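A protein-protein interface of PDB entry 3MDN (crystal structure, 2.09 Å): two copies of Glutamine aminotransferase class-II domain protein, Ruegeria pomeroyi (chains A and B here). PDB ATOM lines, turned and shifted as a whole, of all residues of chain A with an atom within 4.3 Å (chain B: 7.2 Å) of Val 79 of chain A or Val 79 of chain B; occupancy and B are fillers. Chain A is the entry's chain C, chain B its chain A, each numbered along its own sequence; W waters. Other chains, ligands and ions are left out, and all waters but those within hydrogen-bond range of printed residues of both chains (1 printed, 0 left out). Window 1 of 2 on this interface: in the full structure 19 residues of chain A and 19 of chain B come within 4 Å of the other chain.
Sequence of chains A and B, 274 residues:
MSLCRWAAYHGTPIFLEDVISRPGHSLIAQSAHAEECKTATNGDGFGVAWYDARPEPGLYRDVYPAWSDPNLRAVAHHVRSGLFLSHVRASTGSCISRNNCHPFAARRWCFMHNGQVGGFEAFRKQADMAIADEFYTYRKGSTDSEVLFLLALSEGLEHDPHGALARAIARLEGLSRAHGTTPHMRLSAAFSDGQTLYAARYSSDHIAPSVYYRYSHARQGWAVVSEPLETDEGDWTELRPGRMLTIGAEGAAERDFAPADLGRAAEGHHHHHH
Water W1 bridges the backbone carbonyl oxygen (O) of His 78 of chain A (2.8 Å) and the backbone NH (N) of Ala 53 of chain B (2.9 Å).
Trp 50 of chain A touches His 78 of chain B, and with the chains exchanged His 78 of chain A touches Trp 50 of chain B.
Val 75 of chain A touches its own counterpart, Val 75 of chain B.
Val 79 of chain B touches its own counterpart, Val 79 of chain A.
10 positions are printed for both chains.
The side-chain carboxylate of Asp 52 of chain B lies within salt-bridge range of the guanidinium group of Arg 80 of chain A (3.9 Å).
The backbone carbonyl oxygen (O) of His 77 of chain A is in hydrogen-bond range of the guanidinium group (NE) of Arg 54 of chain B, at 2.7 Å.
Among the printed residues, pairs that only touch across the chains: Arg 80 of chain A with Ala 53 of chain B, Phe 15 of chain A with Arg 54 of chain B, His 78 of chain A with Asp 52 of chain B, Phe 15 of chain A with Ala 53 of chain B, His 78 of chain A with Trp 50 of chain B, His 78 of chain A with Arg 54 of chain B, Val 75 of chain A with Val 75 of chain B, Trp 50 of chain A with His 78 of chain B and Val 79 of chain A with Val 79 of chain B.
The backbone NH of Leu 16 of chain B lies within hydrogen-bond range of the backbone carbonyl oxygen of Val 79 of chain B, 3.2 Å away.
A ring nitrogen (ND1) of His 78 of chain B sits at hydrogen-bond distance from the backbone carbonyl oxygen (O) of Ala 74 of chain B, 3.3 Å away.
O of Val 79 of chain A lies within hydrogen-bond range of N of Leu 16 of chain A (3.1 Å).
Of chain B, only Val 79 (3.9 Å) comes within 4 Å of Val 79 of chain A.
Val 79 of chain B touches one residue of chain A.
Printed residues of chain A within 4 Å of Val 75 of chain B: Val 75 (3.9 Å).
Of the printed residues of chain B, Phe 15 of chain A touches Ala 53 (3.8 Å) and Arg 54 (3.4 Å).
Of the printed residues of chain B, His 77 of chain A touches Arg 54.
Printed residues of chain A within 4 Å of Ala 53 of chain B: Phe 15 (3.8 Å) and Arg 80 (3.3 Å).
Of the printed residues of chain A, His 78 of chain B touches Trp 50.
Phe 15 of chain B touches none of the printed residues of chain A.
The nearest printed residue of chain A that does not touch Val 79 of chain B is Trp 50 of chain A (4.7 Å).
The nearest printed residue of chain B that does not touch Trp 50 of chain A is Ala 74 of chain B (4.6 Å).
Of the 19 printed residues of chain B, 7 touch a printed residue of chain A.
Hydrophobic or aromatic side chains of chain A within 4 Å of the printed part of chain B: Phe 15, Trp 50, Val 75, His 77, His 78 and Val 79.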
ATOM      1  N   ILE A  14      27.339  23.316 -10.650  1.00  0.00           N
ATOM      2  CA  ILE A  14      26.648  22.018 -10.625  1.00  0.00           C
ATOM      3  C   ILE A  14      25.243  22.274 -10.087  1.00  0.00           C
ATOM      4  O   ILE A  14      25.006  23.313  -9.465  1.00  0.00           O
ATOM      5  CB  ILE A  14      27.376  20.982  -9.684  1.00  0.00           C
ATOM      6  CG1 ILE A  14      27.646  21.610  -8.311  1.00  0.00           C
ATOM      7  CG2 ILE A  14      28.648  20.426 -10.374  1.00  0.00           C
ATOM      8  CD1 ILE A  14      28.110  20.653  -7.149  1.00  0.00           C
ATOM      9  N   PHE A  15      24.317  21.354 -10.337  1.00  0.00           N
ATOM     10  CA  PHE A  15      23.006  21.428  -9.699  1.00  0.00           C
ATOM     11  C   PHE A  15      23.223  21.340  -8.184  1.00  0.00           C
ATOM     12  O   PHE A  15      24.123  20.616  -7.720  1.00  0.00           O
ATOM     13  CB  PHE A  15      22.086  20.306 -10.218  1.00  0.00           C
ATOM     14  CG  PHE A  15      21.566  20.532 -11.628  1.00  0.00           C
ATOM     15  CD1 PHE A  15      20.514  21.430 -11.872  1.00  0.00           C
ATOM     16  CD2 PHE A  15      22.102  19.835 -12.710  1.00  0.00           C
ATOM     17  CE1 PHE A  15      20.031  21.631 -13.164  1.00  0.00           C
ATOM     18  CE2 PHE A  15      21.628  20.021 -14.008  1.00  0.00           C
ATOM     19  CZ  PHE A  15      20.597  20.925 -14.248  1.00  0.00           C
ATOM     20  N   LEU A  16      22.454  22.095  -7.391  1.00  0.00           N
ATOM     21  CA  LEU A  16      22.663  22.101  -5.935  1.00  0.00           C
ATOM     22  C   LEU A  16      22.524  20.677  -5.388  1.00  0.00           C
ATOM     23  O   LEU A  16      23.190  20.308  -4.421  1.00  0.00           O
ATOM     24  CB  LEU A  16      21.675  23.043  -5.221  1.00  0.00           C
ATOM     25  CG  LEU A  16      21.468  24.492  -5.718  1.00  0.00           C
ATOM     26  CD1 LEU A  16      20.409  25.272  -4.873  1.00  0.00           C
ATOM     27  CD2 LEU A  16      22.802  25.260  -5.764  1.00  0.00           C
ATOM     28  N   TRP A  50      23.193  30.249  -2.237  1.00  0.00           N
ATOM     29  CA  TRP A  50      23.913  29.984  -3.500  1.00  0.00           C
ATOM     30  C   TRP A  50      24.207  31.264  -4.250  1.00  0.00           C
ATOM     31  O   TRP A  50      23.441  32.214  -4.185  1.00  0.00           O
ATOM     32  CB  TRP A  50      23.127  29.003  -4.383  1.00  0.00           C
ATOM     33  CG  TRP A  50      22.002  29.604  -5.152  1.00  0.00           C
ATOM     34  CD1 TRP A  50      22.041  30.072  -6.456  1.00  0.00           C
ATOM     35  CD2 TRP A  50      20.661  29.797  -4.696  1.00  0.00           C
ATOM     36  NE1 TRP A  50      20.802  30.543  -6.803  1.00  0.00           N
ATOM     37  CE2 TRP A  50      19.938  30.375  -5.755  1.00  0.00           C
ATOM     38  CE3 TRP A  50      19.999  29.526  -3.486  1.00  0.00           C
ATOM     39  CZ2 TRP A  50      18.577  30.697  -5.649  1.00  0.00           C
ATOM     40  CZ3 TRP A  50      18.654  29.848  -3.372  1.00  0.00           C
ATOM     41  CH2 TRP A  50      17.952  30.421  -4.453  1.00  0.00           C
ATOM     42  N   VAL A  75      13.977  23.265  -6.472  1.00  0.00           N
ATOM     43  CA  VAL A  75      15.071  24.203  -6.518  1.00  0.00           C
ATOM     44  C   VAL A  75      16.440  23.502  -6.645  1.00  0.00           C
ATOM     45  O   VAL A  75      17.278  23.915  -7.469  1.00  0.00           O
ATOM     46  CB  VAL A  75      14.995  25.160  -5.307  1.00  0.00           C
ATOM     47  CG1 VAL A  75      16.292  25.960  -5.114  1.00  0.00           C
ATOM     48  CG2 VAL A  75      13.777  26.076  -5.455  1.00  0.00           C
ATOM     49  N   ALA A  76      16.662  22.451  -5.849  1.00  0.00           N
ATOM     50  CA  ALA A  76      17.945  21.756  -5.868  1.00  0.00           C
ATOM     51  C   ALA A  76      18.123  21.007  -7.174  1.00  0.00           C
ATOM     52  O   ALA A  76      19.249  20.853  -7.638  1.00  0.00           O
ATOM     53  CB  ALA A  76      18.094  20.810  -4.675  1.00  0.00           C
ATOM     54  N   HIS A  77      17.005  20.541  -7.755  1.00  0.00           N
ATOM     55  CA  HIS A  77      17.041  19.772  -8.977  1.00  0.00           C
ATOM     56  C   HIS A  77      17.235  20.717 -10.190  1.00  0.00           C
ATOM     57  O   HIS A  77      17.700  20.288 -11.235  1.00  0.00           O
ATOM     58  CB  HIS A  77      15.759  18.937  -9.107  1.00  0.00           C
ATOM     59  CG  HIS A  77      15.708  18.054 -10.322  1.00  0.00           C
ATOM     60  ND1 HIS A  77      16.670  17.108 -10.597  1.00  0.00           N
ATOM     61  CD2 HIS A  77      14.799  17.960 -11.326  1.00  0.00           C
ATOM     62  CE1 HIS A  77      16.362  16.471 -11.712  1.00  0.00           C
ATOM     63  NE2 HIS A  77      15.240  16.980 -12.185  1.00  0.00           N
ATOM     64  N   HIS A  78      16.901  22.002 -10.035  1.00  0.00           N
ATOM     65  CA  HIS A  78      16.842  22.918 -11.184  1.00  0.00           C
ATOM     66  C   HIS A  78      17.833  24.096 -11.218  1.00  0.00           C
ATOM     67  O   HIS A  78      18.097  24.637 -12.276  1.00  0.00           O
ATOM     68  CB  HIS A  78      15.413  23.446 -11.409  1.00  0.00           C
ATOM     69  CG  HIS A  78      14.556  22.527 -12.215  1.00  0.00           C
ATOM     70  ND1 HIS A  78      13.638  21.669 -11.646  1.00  0.00           N
ATOM     71  CD2 HIS A  78      14.482  22.325 -13.544  1.00  0.00           C
ATOM     72  CE1 HIS A  78      13.040  20.972 -12.591  1.00  0.00           C
ATOM     73  NE2 HIS A  78      13.532  21.353 -13.755  1.00  0.00           N
ATOM     74  N   VAL A  79      18.336  24.505 -10.074  1.00  0.00           N
ATOM     75  CA  VAL A  79      19.296  25.607  -9.976  1.00  0.00           C
ATOM     76  C   VAL A  79      20.739  25.092  -9.948  1.00  0.00           C
ATOM     77  O   VAL A  79      21.061  24.151  -9.214  1.00  0.00           O
ATOM     78  CB  VAL A  79      19.081  26.417  -8.662  1.00  0.00           C
ATOM     79  CG1 VAL A  79      20.225  27.398  -8.456  1.00  0.00           C
ATOM     80  CG2 VAL A  79      17.716  27.151  -8.749  1.00  0.00           C
ATOM     81  N   ARG A  80      21.591  25.717 -10.763  1.00  0.00           N
ATOM     82  CA  ARG A  80      23.008  25.394 -10.871  1.00  0.00           C
ATOM     83  C   ARG A  80      23.829  26.511 -10.258  1.00  0.00           C
ATOM     84  O   ARG A  80      23.495  27.662 -10.422  1.00  0.00           O
ATOM     85  CB  ARG A  80      23.391  25.238 -12.358  1.00  0.00           C
ATOM     86  CG  ARG A  80      22.840  23.956 -12.997  1.00  0.00           C
ATOM     87  CD  ARG A  80      23.132  23.899 -14.529  1.00  0.00           C
ATOM     88  NE  ARG A  80      22.469  25.007 -15.238  1.00  0.00           N
ATOM     89  CZ  ARG A  80      22.401  25.110 -16.559  1.00  0.00           C
ATOM     90  NH1 ARG A  80      22.935  24.155 -17.320  1.00  0.00           N
ATOM     91  NH2 ARG A  80      21.779  26.136 -17.121  1.00  0.00           N
ATOM     92  N   ILE B  14      14.541  36.384 -18.392  1.00  0.00           N
ATOM     93  CA  ILE B  14      14.508  37.413 -17.352  1.00  0.00           C
ATOM     94  C   ILE B  14      14.389  36.794 -15.940  1.00  0.00           C
ATOM     95  O   ILE B  14      14.060  35.613 -15.791  1.00  0.00           O
ATOM     96  CB  ILE B  14      13.341  38.370 -17.582  1.00  0.00           C
ATOM     97  CG1 ILE B  14      12.052  37.572 -17.722  1.00  0.00           C
ATOM     98  CG2 ILE B  14      13.581  39.167 -18.835  1.00  0.00           C
ATOM     99  CD1 ILE B  14      10.758  38.409 -17.773  1.00  0.00           C
ATOM    100  N   PHE B  15      14.671  37.576 -14.906  1.00  0.00           N
ATOM    101  CA  PHE B  15      14.440  37.078 -13.553  1.00  0.00           C
ATOM    102  C   PHE B  15      12.937  36.956 -13.438  1.00  0.00           C
ATOM    103  O   PHE B  15      12.198  37.784 -13.995  1.00  0.00           O
ATOM    104  CB  PHE B  15      14.947  38.045 -12.495  1.00  0.00           C
ATOM    105  CG  PHE B  15      16.432  38.190 -12.470  1.00  0.00           C
ATOM    106  CD1 PHE B  15      17.228  37.216 -11.869  1.00  0.00           C
ATOM    107  CD2 PHE B  15      17.036  39.311 -13.006  1.00  0.00           C
ATOM    108  CE1 PHE B  15      18.611  37.358 -11.835  1.00  0.00           C
ATOM    109  CE2 PHE B  15      18.411  39.464 -12.969  1.00  0.00           C
ATOM    110  CZ  PHE B  15      19.204  38.489 -12.390  1.00  0.00           C
ATOM    111  N   LEU B  16      12.483  35.933 -12.732  1.00  0.00           N
ATOM    112  CA  LEU B  16      11.056  35.663 -12.632  1.00  0.00           C
ATOM    113  C   LEU B  16      10.304  36.877 -12.060  1.00  0.00           C
ATOM    114  O   LEU B  16       9.230  37.211 -12.543  1.00  0.00           O
ATOM    115  CB  LEU B  16      10.780  34.405 -11.812  1.00  0.00           C
ATOM    116  CG  LEU B  16      11.602  33.148 -12.173  1.00  0.00           C
ATOM    117  CD1 LEU B  16      11.275  31.971 -11.235  1.00  0.00           C
ATOM    118  CD2 LEU B  16      11.417  32.755 -13.688  1.00  0.00           C
ATOM    119  N   GLU B  17      10.890  37.553 -11.074  1.00  0.00           N
ATOM    120  CA  GLU B  17      10.233  38.720 -10.486  1.00  0.00           C
ATOM    121  C   GLU B  17       9.992  39.886 -11.475  1.00  0.00           C
ATOM    122  O   GLU B  17       9.159  40.740 -11.204  1.00  0.00           O
ATOM    123  CB  GLU B  17      11.039  39.253  -9.318  1.00  0.00           C
ATOM    124  CG  GLU B  17      12.310  39.938  -9.738  1.00  0.00           C
ATOM    125  CD  GLU B  17      13.156  40.365  -8.540  1.00  0.00           C
ATOM    126  OE1 GLU B  17      12.653  40.279  -7.409  1.00  0.00           O
ATOM    127  OE2 GLU B  17      14.310  40.780  -8.725  1.00  0.00           O
ATOM    128  N   TRP B  50       8.895  27.008 -14.351  1.00  0.00           N
ATOM    129  CA  TRP B  50       9.843  27.676 -15.252  1.00  0.00           C
ATOM    130  C   TRP B  50      10.751  26.678 -15.899  1.00  0.00           C
ATOM    131  O   TRP B  50      11.036  25.620 -15.332  1.00  0.00           O
ATOM    132  CB  TRP B  50      10.703  28.709 -14.505  1.00  0.00           C
ATOM    133  CG  TRP B  50      11.857  28.132 -13.699  1.00  0.00           C
ATOM    134  CD1 TRP B  50      13.174  28.020 -14.087  1.00  0.00           C
ATOM    135  CD2 TRP B  50      11.796  27.619 -12.359  1.00  0.00           C
ATOM    136  NE1 TRP B  50      13.922  27.449 -13.081  1.00  0.00           N
ATOM    137  CE2 TRP B  50      13.111  27.204 -12.006  1.00  0.00           C
ATOM    138  CE3 TRP B  50      10.758  27.462 -11.428  1.00  0.00           C
ATOM    139  CZ2 TRP B  50      13.410  26.645 -10.770  1.00  0.00           C
ATOM    140  CZ3 TRP B  50      11.045  26.892 -10.199  1.00  0.00           C
ATOM    141  CH2 TRP B  50      12.369  26.481  -9.876  1.00  0.00           C
ATOM    142  N   TYR B  51      11.221  27.023 -17.091  1.00  0.00           N
ATOM    143  CA  TYR B  51      12.168  26.155 -17.797  1.00  0.00           C
ATOM    144  C   TYR B  51      13.525  26.844 -17.747  1.00  0.00           C
ATOM    145  O   TYR B  51      13.631  28.054 -17.943  1.00  0.00           O
ATOM    146  CB  TYR B  51      11.737  25.925 -19.280  1.00  0.00           C
ATOM    147  CG  TYR B  51      10.439  25.156 -19.392  1.00  0.00           C
ATOM    148  CD1 TYR B  51       9.220  25.827 -19.330  1.00  0.00           C
ATOM    149  CD2 TYR B  51      10.429  23.759 -19.511  1.00  0.00           C
ATOM    150  CE1 TYR B  51       8.025  25.139 -19.435  1.00  0.00           C
ATOM    151  CE2 TYR B  51       9.213  23.045 -19.592  1.00  0.00           C
ATOM    152  CZ  TYR B  51       8.015  23.763 -19.556  1.00  0.00           C
ATOM    153  OH  TYR B  51       6.791  23.145 -19.633  1.00  0.00           O
ATOM    154  N   ASP B  52      14.545  26.039 -17.508  1.00  0.00           N
ATOM    155  CA  ASP B  52      15.913  26.512 -17.452  1.00  0.00           C
ATOM    156  C   ASP B  52      16.825  25.487 -18.102  1.00  0.00           C
ATOM    157  O   ASP B  52      17.081  25.548 -19.297  1.00  0.00           O
ATOM    158  CB  ASP B  52      16.347  26.720 -15.987  1.00  0.00           C
ATOM    159  CG  ASP B  52      17.728  27.361 -15.883  1.00  0.00           C
ATOM    160  OD1 ASP B  52      18.251  27.838 -16.921  1.00  0.00           O
ATOM    161  OD2 ASP B  52      18.287  27.377 -14.769  1.00  0.00           O
ATOM    162  N   ALA B  53      17.315  24.536 -17.318  1.00  0.00           N
ATOM    163  CA  ALA B  53      18.326  23.623 -17.847  1.00  0.00           C
ATOM    164  C   ALA B  53      17.768  22.243 -18.195  1.00  0.00           C
ATOM    165  O   ALA B  53      18.492  21.406 -18.723  1.00  0.00           O
ATOM    166  CB  ALA B  53      19.504  23.479 -16.871  1.00  0.00           C
ATOM    167  N   ARG B  54      16.504  21.978 -17.882  1.00  0.00           N
ATOM    168  CA  ARG B  54      16.005  20.626 -18.115  1.00  0.00           C
ATOM    169  C   ARG B  54      14.791  20.677 -19.046  1.00  0.00           C
ATOM    170  O   ARG B  54      14.108  21.708 -19.110  1.00  0.00           O
ATOM    171  CB  ARG B  54      15.629  19.935 -16.785  1.00  0.00           C
ATOM    172  CG  ARG B  54      16.687  19.986 -15.636  1.00  0.00           C
ATOM    173  CD  ARG B  54      16.494  18.794 -14.679  1.00  0.00           C
ATOM    174  NE  ARG B  54      17.383  18.756 -13.494  1.00  0.00           N
ATOM    175  CZ  ARG B  54      18.502  18.043 -13.415  1.00  0.00           C
ATOM    176  NH1 ARG B  54      18.889  17.326 -14.456  1.00  0.00           N
ATOM    177  NH2 ARG B  54      19.235  18.029 -12.289  1.00  0.00           N
ATOM    178  N   ARG B  73      10.434  34.672  -2.716  1.00  0.00           N
ATOM    179  CA  ARG B  73      11.058  35.927  -3.045  1.00  0.00           C
ATOM    180  C   ARG B  73      12.503  35.728  -3.526  1.00  0.00           C
ATOM    181  O   ARG B  73      12.944  36.314  -4.530  1.00  0.00           O
ATOM    182  CB  ARG B  73      10.992  36.863  -1.841  1.00  0.00           C
ATOM    183  CG  ARG B  73      11.520  38.257  -2.135  1.00  0.00           C
ATOM    184  CD  ARG B  73      11.062  39.301  -1.082  1.00  0.00           C
ATOM    185  NE  ARG B  73      10.978  40.647  -1.677  1.00  0.00           N
ATOM    186  CZ  ARG B  73      10.312  40.924  -2.803  1.00  0.00           C
ATOM    187  NH1 ARG B  73       9.680  39.961  -3.458  1.00  0.00           N
ATOM    188  NH2 ARG B  73      10.279  42.156  -3.288  1.00  0.00           N
ATOM    189  N   ALA B  74      13.249  34.899  -2.808  1.00  0.00           N
ATOM    190  CA  ALA B  74      14.613  34.619  -3.220  1.00  0.00           C
ATOM    191  C   ALA B  74      14.675  33.879  -4.565  1.00  0.00           C
ATOM    192  O   ALA B  74      15.526  34.187  -5.379  1.00  0.00           O
ATOM    193  CB  ALA B  74      15.358  33.857  -2.122  1.00  0.00           C
ATOM    194  N   VAL B  75      13.806  32.895  -4.787  1.00  0.00           N
ATOM    195  CA  VAL B  75      13.749  32.232  -6.083  1.00  0.00           C
ATOM    196  C   VAL B  75      13.444  33.235  -7.238  1.00  0.00           C
ATOM    197  O   VAL B  75      14.144  33.253  -8.263  1.00  0.00           O
ATOM    198  CB  VAL B  75      12.723  31.077  -6.095  1.00  0.00           C
ATOM    199  CG1 VAL B  75      12.425  30.626  -7.534  1.00  0.00           C
ATOM    200  CG2 VAL B  75      13.198  29.910  -5.237  1.00  0.00           C
ATOM    201  N   ALA B  76      12.437  34.094  -7.050  1.00  0.00           N
ATOM    202  CA  ALA B  76      12.026  35.020  -8.125  1.00  0.00           C
ATOM    203  C   ALA B  76      13.057  36.105  -8.345  1.00  0.00           C
ATOM    204  O   ALA B  76      13.151  36.658  -9.435  1.00  0.00           O
ATOM    205  CB  ALA B  76      10.647  35.640  -7.850  1.00  0.00           C
ATOM    206  N   HIS B  77      13.842  36.401  -7.324  1.00  0.00           N
ATOM    207  CA  HIS B  77      14.848  37.447  -7.436  1.00  0.00           C
ATOM    208  C   HIS B  77      16.145  36.886  -8.053  1.00  0.00           C
ATOM    209  O   HIS B  77      16.937  37.647  -8.613  1.00  0.00           O
ATOM    210  CB  HIS B  77      15.086  38.083  -6.055  1.00  0.00           C
ATOM    211  CG  HIS B  77      16.164  39.132  -6.002  1.00  0.00           C
ATOM    212  ND1 HIS B  77      16.090  40.324  -6.695  1.00  0.00           N
ATOM    213  CD2 HIS B  77      17.292  39.212  -5.247  1.00  0.00           C
ATOM    214  CE1 HIS B  77      17.152  41.064  -6.418  1.00  0.00           C
ATOM    215  NE2 HIS B  77      17.897  40.412  -5.545  1.00  0.00           N
ATOM    216  N   HIS B  78      16.354  35.568  -7.977  1.00  0.00           N
ATOM    217  CA  HIS B  78      17.638  35.006  -8.391  1.00  0.00           C
ATOM    218  C   HIS B  78      17.598  34.077  -9.613  1.00  0.00           C
ATOM    219  O   HIS B  78      18.617  33.856 -10.254  1.00  0.00           O
ATOM    220  CB  HIS B  78      18.335  34.274  -7.213  1.00  0.00           C
ATOM    221  CG  HIS B  78      19.045  35.193  -6.255  1.00  0.00           C
ATOM    222  ND1 HIS B  78      18.449  35.697  -5.114  1.00  0.00           N
ATOM    223  CD2 HIS B  78      20.298  35.703  -6.276  1.00  0.00           C
ATOM    224  CE1 HIS B  78      19.305  36.476  -4.479  1.00  0.00           C
ATOM    225  NE2 HIS B  78      20.436  36.490  -5.162  1.00  0.00           N
ATOM    226  N   VAL B  79      16.450  33.496  -9.913  1.00  0.00           N
ATOM    227  CA  VAL B  79      16.395  32.554 -11.013  1.00  0.00           C
ATOM    228  C   VAL B  79      15.971  33.296 -12.285  1.00  0.00           C
ATOM    229  O   VAL B  79      15.026  34.081 -12.260  1.00  0.00           O
ATOM    230  CB  VAL B  79      15.412  31.384 -10.708  1.00  0.00           C
ATOM    231  CG1 VAL B  79      15.159  30.491 -11.969  1.00  0.00           C
ATOM    232  CG2 VAL B  79      15.935  30.586  -9.536  1.00  0.00           C
ATOM    233  N   ARG B  80      16.688  33.032 -13.381  1.00  0.00           N
ATOM    234  CA  ARG B  80      16.373  33.576 -14.713  1.00  0.00           C
ATOM    235  C   ARG B  80      15.780  32.501 -15.644  1.00  0.00           C
ATOM    236  O   ARG B  80      16.225  31.370 -15.632  1.00  0.00           O
ATOM    237  CB  ARG B  80      17.636  34.195 -15.352  1.00  0.00           C
ATOM    238  CG  ARG B  80      17.736  35.731 -15.203  1.00  0.00           C
ATOM    239  CD  ARG B  80      19.081  36.229 -15.745  1.00  0.00           C
ATOM    240  NE  ARG B  80      20.085  35.243 -15.343  1.00  0.00           N
ATOM    241  CZ  ARG B  80      21.402  35.403 -15.412  1.00  0.00           C
ATOM    242  NH1 ARG B  80      21.923  36.541 -15.867  1.00  0.00           N
ATOM    243  NH2 ARG B  80      22.197  34.411 -15.016  1.00  0.00           N
ATOM    244  N   SER B  81      14.798  32.874 -16.460  1.00  0.00           N
ATOM    245  CA  SER B  81      14.164  31.943 -17.381  1.00  0.00           C
ATOM    246  C   SER B  81      13.524  32.655 -18.588  1.00  0.00           C
ATOM    247  O   SER B  81      12.976  33.783 -18.492  1.00  0.00           O
ATOM    248  CB  SER B  81      13.094  31.124 -16.640  1.00  0.00           C
ATOM    249  OG  SER B  81      12.321  30.319 -17.518  1.00  0.00           O
ATOM    250  N   PHE B  84       8.269  30.755 -18.655  1.00  0.00           N
ATOM    251  CA  PHE B  84       7.775  30.432 -17.322  1.00  0.00           C
ATOM    252  C   PHE B  84       6.331  30.875 -17.175  1.00  0.00           C
ATOM    253  O   PHE B  84       5.859  31.698 -17.965  1.00  0.00           O
ATOM    254  CB  PHE B  84       8.654  31.006 -16.193  1.00  0.00           C
ATOM    255  CG  PHE B  84       8.791  32.533 -16.169  1.00  0.00           C
ATOM    256  CD1 PHE B  84       7.946  33.324 -15.361  1.00  0.00           C
ATOM    257  CD2 PHE B  84       9.824  33.173 -16.873  1.00  0.00           C
ATOM    258  CE1 PHE B  84       8.128  34.752 -15.322  1.00  0.00           C
ATOM    259  CE2 PHE B  84      10.038  34.534 -16.801  1.00  0.00           C
ATOM    260  CZ  PHE B  84       9.176  35.345 -16.043  1.00  0.00           C
HETATM  261  O   HOH W   1      16.696  23.749 -14.554  1.00  0.00           O
